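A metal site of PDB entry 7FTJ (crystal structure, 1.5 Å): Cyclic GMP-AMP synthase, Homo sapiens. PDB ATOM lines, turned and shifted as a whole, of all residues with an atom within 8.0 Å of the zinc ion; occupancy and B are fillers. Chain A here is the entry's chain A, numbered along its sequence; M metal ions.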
ATOM      1  N   LEU A 227       1.494  13.836  13.926  1.00  0.00           N
ATOM      2  CA  LEU A 227       1.509  15.291  14.125  1.00  0.00           C
ATOM      3  C   LEU A 227       1.700  15.666  15.580  1.00  0.00           C
ATOM      4  O   LEU A 227       2.353  16.683  15.870  1.00  0.00           O
ATOM      5  CB  LEU A 227       0.242  15.921  13.550  1.00  0.00           C
ATOM      6  CG  LEU A 227       0.277  16.185  12.054  1.00  0.00           C
ATOM      7  CD1 LEU A 227      -1.128  16.538  11.569  1.00  0.00           C
ATOM      8  CD2 LEU A 227       1.242  17.332  11.775  1.00  0.00           C
ATOM      9  N   ASN A 229       3.320  13.803  17.766  1.00  0.00           N
ATOM     10  CA  ASN A 229       4.559  13.188  18.255  1.00  0.00           C
ATOM     11  C   ASN A 229       5.474  13.147  17.036  1.00  0.00           C
ATOM     12  O   ASN A 229       5.739  12.117  16.421  1.00  0.00           O
ATOM     13  CB  ASN A 229       4.269  11.793  18.839  1.00  0.00           C
ATOM     14  CG  ASN A 229       5.466  11.206  19.549  1.00  0.00           C
ATOM     15  OD1 ASN A 229       6.492  11.855  19.703  1.00  0.00           O
ATOM     16  ND2 ASN A 229       5.306   9.961  20.014  1.00  0.00           N
ATOM     17  N   HIS A 230       5.959  14.325  16.653  1.00  0.00           N
ATOM     18  CA  HIS A 230       6.406  14.590  15.304  1.00  0.00           C
ATOM     19  C   HIS A 230       7.901  14.765  15.133  1.00  0.00           C
ATOM     20  O   HIS A 230       8.335  15.005  14.000  1.00  0.00           O
ATOM     21  CB  HIS A 230       5.721  15.874  14.792  1.00  0.00           C
ATOM     22  CG  HIS A 230       6.058  17.076  15.627  1.00  0.00           C
ATOM     23  ND1 HIS A 230       5.104  17.794  16.325  1.00  0.00           N
ATOM     24  CD2 HIS A 230       7.260  17.608  15.954  1.00  0.00           C
ATOM     25  CE1 HIS A 230       5.712  18.754  17.001  1.00  0.00           C
ATOM     26  NE2 HIS A 230       7.021  18.666  16.807  1.00  0.00           N
ATOM     27  N   GLY A 231       8.695  14.709  16.206  1.00  0.00           N
ATOM     28  CA  GLY A 231      10.114  14.968  16.109  1.00  0.00           C
ATOM     29  C   GLY A 231      10.907  13.686  15.948  1.00  0.00           C
ATOM     30  O   GLY A 231      10.471  12.595  16.331  1.00  0.00           O
ATOM     31  N   LYS A 232      12.117  13.819  15.404  1.00  0.00           N
ATOM     32  CA  LYS A 232      13.114  12.768  15.620  1.00  0.00           C
ATOM     33  C   LYS A 232      13.411  12.602  17.113  1.00  0.00           C
ATOM     34  O   LYS A 232      13.424  11.478  17.636  1.00  0.00           O
ATOM     35  CB  LYS A 232      14.386  13.054  14.827  1.00  0.00           C
ATOM     36  CG  LYS A 232      15.482  12.015  15.136  1.00  0.00           C
ATOM     37  CD  LYS A 232      16.694  12.146  14.215  1.00  0.00           C
ATOM     38  CE  LYS A 232      16.333  11.844  12.771  1.00  0.00           C
ATOM     39  NZ  LYS A 232      15.631  10.513  12.688  1.00  0.00           N
ATOM     40  N   SER A 233      13.603  13.711  17.824  1.00  0.00           N
ATOM     41  CA  SER A 233      13.732  13.637  19.276  1.00  0.00           C
ATOM     42  C   SER A 233      12.384  13.362  19.930  1.00  0.00           C
ATOM     43  O   SER A 233      11.379  14.004  19.620  1.00  0.00           O
ATOM     44  CB  SER A 233      14.249  14.960  19.821  1.00  0.00           C
ATOM     45  OG  SER A 233      14.223  14.963  21.240  1.00  0.00           O
ATOM     46  N   THR A 235      11.631  14.315  22.743  1.00  0.00           N
ATOM     47  CA  THR A 235      11.290  15.524  23.481  1.00  0.00           C
ATOM     48  C   THR A 235      11.136  16.752  22.586  1.00  0.00           C
ATOM     49  O   THR A 235      11.126  17.872  23.101  1.00  0.00           O
ATOM     50  CB  THR A 235      12.272  15.776  24.636  1.00  0.00           C
ATOM     51  OG1 THR A 235      13.628  15.643  24.181  1.00  0.00           O
ATOM     52  CG2 THR A 235      12.029  14.819  25.805  1.00  0.00           C
ATOM     53  N   CYS A 236      10.982  16.563  21.275  1.00  0.00           N
ATOM     54  CA  CYS A 236      10.713  17.691  20.383  1.00  0.00           C
ATOM     55  C   CYS A 236       9.465  18.431  20.850  1.00  0.00           C
ATOM     56  O   CYS A 236       8.429  17.831  21.155  1.00  0.00           O
ATOM     57  CB  CYS A 236      10.521  17.188  18.941  1.00  0.00           C
ATOM     58  SG  CYS A 236      10.479  18.522  17.677  1.00  0.00           S
ATOM     59  N   CYS A 237       9.596  19.754  20.989  1.00  0.00           N
ATOM     60  CA  CYS A 237       8.518  20.622  21.453  1.00  0.00           C
ATOM     61  C   CYS A 237       8.081  20.351  22.903  1.00  0.00           C
ATOM     62  O   CYS A 237       7.005  20.810  23.332  1.00  0.00           O
ATOM     63  CB  CYS A 237       7.333  20.661  20.474  1.00  0.00           C
ATOM     64  SG  CYS A 237       7.758  21.419  18.867  1.00  0.00           S
ATOM     65  N   GLU A 238       8.895  19.654  23.706  1.00  0.00           N
ATOM     66  CA  GLU A 238       8.644  19.537  25.139  1.00  0.00           C
ATOM     67  C   GLU A 238       9.497  20.485  25.973  1.00  0.00           C
ATOM     68  O   GLU A 238       9.360  20.516  27.209  1.00  0.00           O
ATOM     69  CB  GLU A 238       8.803  18.087  25.639  1.00  0.00           C
ATOM     70  CG  GLU A 238       7.725  17.131  25.123  1.00  0.00           C
ATOM     71  CD  GLU A 238       7.640  15.816  25.891  1.00  0.00           C
ATOM     72  OE1 GLU A 238       8.503  15.537  26.761  1.00  0.00           O
ATOM     73  OE2 GLU A 238       6.693  15.053  25.622  1.00  0.00           O
ATOM     74  N   ASN A 239      10.367  21.266  25.340  1.00  0.00           N
ATOM     75  CA  ASN A 239      11.231  22.201  26.050  1.00  0.00           C
ATOM     76  C   ASN A 239      11.671  23.304  25.086  1.00  0.00           C
ATOM     77  O   ASN A 239      11.541  23.172  23.861  1.00  0.00           O
ATOM     78  CB  ASN A 239      12.439  21.509  26.668  1.00  0.00           C
ATOM     79  CG  ASN A 239      13.326  20.872  25.626  1.00  0.00           C
ATOM     80  OD1 ASN A 239      14.026  21.564  24.884  1.00  0.00           O
ATOM     81  ND2 ASN A 239      13.281  19.555  25.552  1.00  0.00           N
ATOM     82  N   GLU A 242      14.166  22.635  22.095  1.00  0.00           N
ATOM     83  CA  GLU A 242      13.715  21.753  21.032  1.00  0.00           C
ATOM     84  C   GLU A 242      12.364  22.203  20.495  1.00  0.00           C
ATOM     85  O   GLU A 242      11.485  21.399  20.153  1.00  0.00           O
ATOM     86  CB  GLU A 242      13.645  20.310  21.504  1.00  0.00           C
ATOM     87  CG  GLU A 242      14.934  19.754  22.024  1.00  0.00           C
ATOM     88  CD  GLU A 242      14.785  18.295  22.358  1.00  0.00           C
ATOM     89  OE1 GLU A 242      14.707  17.503  21.397  1.00  0.00           O
ATOM     90  OE2 GLU A 242      14.674  17.949  23.544  1.00  0.00           O
ATOM     91  N   LYS A 243      12.175  23.508  20.369  1.00  0.00           N
ATOM     92  CA  LYS A 243      10.953  24.038  19.766  1.00  0.00           C
ATOM     93  C   LYS A 243      11.142  24.067  18.255  1.00  0.00           C
ATOM     94  O   LYS A 243      11.960  24.831  17.744  1.00  0.00           O
ATOM     95  CB  LYS A 243      10.649  25.421  20.332  1.00  0.00           C
ATOM     96  CG  LYS A 243       9.312  25.950  19.852  1.00  0.00           C
ATOM     97  CD  LYS A 243       8.600  26.778  20.910  1.00  0.00           C
ATOM     98  CE  LYS A 243       7.394  27.484  20.291  1.00  0.00           C
ATOM     99  NZ  LYS A 243       7.839  28.551  19.347  1.00  0.00           N
ATOM    100  N   CYS A 244      10.416  23.200  17.539  1.00  0.00           N
ATOM    101  CA  CYS A 244      10.514  23.180  16.086  1.00  0.00           C
ATOM    102  C   CYS A 244       9.325  23.934  15.484  1.00  0.00           C
ATOM    103  O   CYS A 244       8.403  24.334  16.200  1.00  0.00           O
ATOM    104  CB  CYS A 244      10.580  21.737  15.566  1.00  0.00           C
ATOM    105  SG  CYS A 244       8.999  20.845  15.346  1.00  0.00           S
ATOM    106  N   CYS A 245       9.365  24.105  14.161  1.00  0.00           N
ATOM    107  CA  CYS A 245       8.318  24.829  13.451  1.00  0.00           C
ATOM    108  C   CYS A 245       7.479  23.940  12.533  1.00  0.00           C
ATOM    109  O   CYS A 245       6.809  24.465  11.654  1.00  0.00           O
ATOM    110  CB  CYS A 245       8.878  26.024  12.678  1.00  0.00           C
ATOM    111  SG  CYS A 245       9.938  25.608  11.305  1.00  0.00           S
ATOM    112  N   ARG A 246       7.500  22.625  12.732  1.00  0.00           N
ATOM    113  CA  ARG A 246       6.695  21.741  11.878  1.00  0.00           C
ATOM    114  C   ARG A 246       5.223  22.129  11.904  1.00  0.00           C
ATOM    115  O   ARG A 246       4.608  22.304  10.846  1.00  0.00           O
ATOM    116  CB  ARG A 246       6.881  20.278  12.333  1.00  0.00           C
ATOM    117  CG  ARG A 246       8.189  19.695  11.882  1.00  0.00           C
ATOM    118  CD  ARG A 246       8.252  18.224  12.269  1.00  0.00           C
ATOM    119  NE  ARG A 246       9.499  17.526  11.964  1.00  0.00           N
ATOM    120  CZ  ARG A 246      10.524  17.396  12.811  1.00  0.00           C
ATOM    121  NH1 ARG A 246      11.580  16.636  12.462  1.00  0.00           N
ATOM    122  NH2 ARG A 246      10.510  18.029  13.985  1.00  0.00           N
ATOM    123  N   LYS A 247       4.633  22.254  13.091  1.00  0.00           N
ATOM    124  CA  LYS A 247       3.196  22.516  13.133  1.00  0.00           C
ATOM    125  C   LYS A 247       2.874  23.901  12.583  1.00  0.00           C
ATOM    126  O   LYS A 247       1.874  24.083  11.872  1.00  0.00           O
ATOM    127  CB  LYS A 247       2.654  22.323  14.540  1.00  0.00           C
ATOM    128  CG  LYS A 247       2.608  20.859  14.926  1.00  0.00           C
ATOM    129  CD  LYS A 247       1.787  20.639  16.182  1.00  0.00           C
ATOM    130  CE  LYS A 247       0.802  19.512  15.987  1.00  0.00           C
ATOM    131  NZ  LYS A 247       0.290  19.039  17.300  1.00  0.00           N
ATOM    132  N   ASP A 292      15.359  17.204  13.271  1.00  0.00           N
ATOM    133  CA  ASP A 292      14.741  18.339  13.940  1.00  0.00           C
ATOM    134  C   ASP A 292      15.498  19.634  13.647  1.00  0.00           C
ATOM    135  O   ASP A 292      14.895  20.705  13.622  1.00  0.00           O
ATOM    136  CB  ASP A 292      14.652  18.133  15.456  1.00  0.00           C
ATOM    137  CG  ASP A 292      13.779  16.956  15.820  1.00  0.00           C
ATOM    138  OD1 ASP A 292      12.901  16.562  15.024  1.00  0.00           O
ATOM    139  OD2 ASP A 292      13.966  16.440  16.942  1.00  0.00           O
ATOM    140  N   TRP A 295      14.086  21.925  11.080  1.00  0.00           N
ATOM    141  CA  TRP A 295      12.817  22.563  11.430  1.00  0.00           C
ATOM    142  C   TRP A 295      12.980  23.488  12.628  1.00  0.00           C
ATOM    143  O   TRP A 295      12.043  23.693  13.411  1.00  0.00           O
ATOM    144  CB  TRP A 295      11.757  21.503  11.757  1.00  0.00           C
ATOM    145  CG  TRP A 295      11.447  20.649  10.606  1.00  0.00           C
ATOM    146  CD1 TRP A 295      12.020  19.447  10.293  1.00  0.00           C
ATOM    147  CD2 TRP A 295      10.480  20.907   9.583  1.00  0.00           C
ATOM    148  NE1 TRP A 295      11.455  18.941   9.155  1.00  0.00           N
ATOM    149  CE2 TRP A 295      10.512  19.812   8.698  1.00  0.00           C
ATOM    150  CE3 TRP A 295       9.572  21.953   9.341  1.00  0.00           C
ATOM    151  CZ2 TRP A 295       9.669  19.736   7.575  1.00  0.00           C
ATOM    152  CZ3 TRP A 295       8.754  21.882   8.234  1.00  0.00           C
ATOM    153  CH2 TRP A 295       8.800  20.770   7.356  1.00  0.00           C
HETATM  154 ZN    ZN M   1       8.565  19.801  17.468  1.00  0.00          ZN
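O of His 230 is in hydrogen-bond range of NE of Arg 246 (3.4 Å).
ND1 of His 230 sits at hydrogen-bond distance from O of Leu 227.
The backbone NH (N) of Cys 237 lies within hydrogen-bond range of the backbone carbonyl oxygen (O) of Glu 242.
The guanidinium group (NH2) of Arg 246 lies close to the side-chain sulfur (SG) of Cys 236 (3.7 Å).
SG of Cys 244 lies close to NH2 of Arg 246.
The zinc ion is bound by a ring nitrogen (NE2) of His 230 (2.0 Å), the side-chain sulfur of Cys 237 (2.3 Å), the side-chain sulfur of Cys 236 (2.3 Å) and the side-chain sulfur of Cys 244 (2.4 Å).
The zinc ion has four donor atoms within binding distance.
Four residues have an atom within 4 Å of the zinc ion: His 230, Cys 236, Cys 237 and Cys 244.
Along chain A the residues within 4 Å of the zinc ion span positions 230 to 244.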
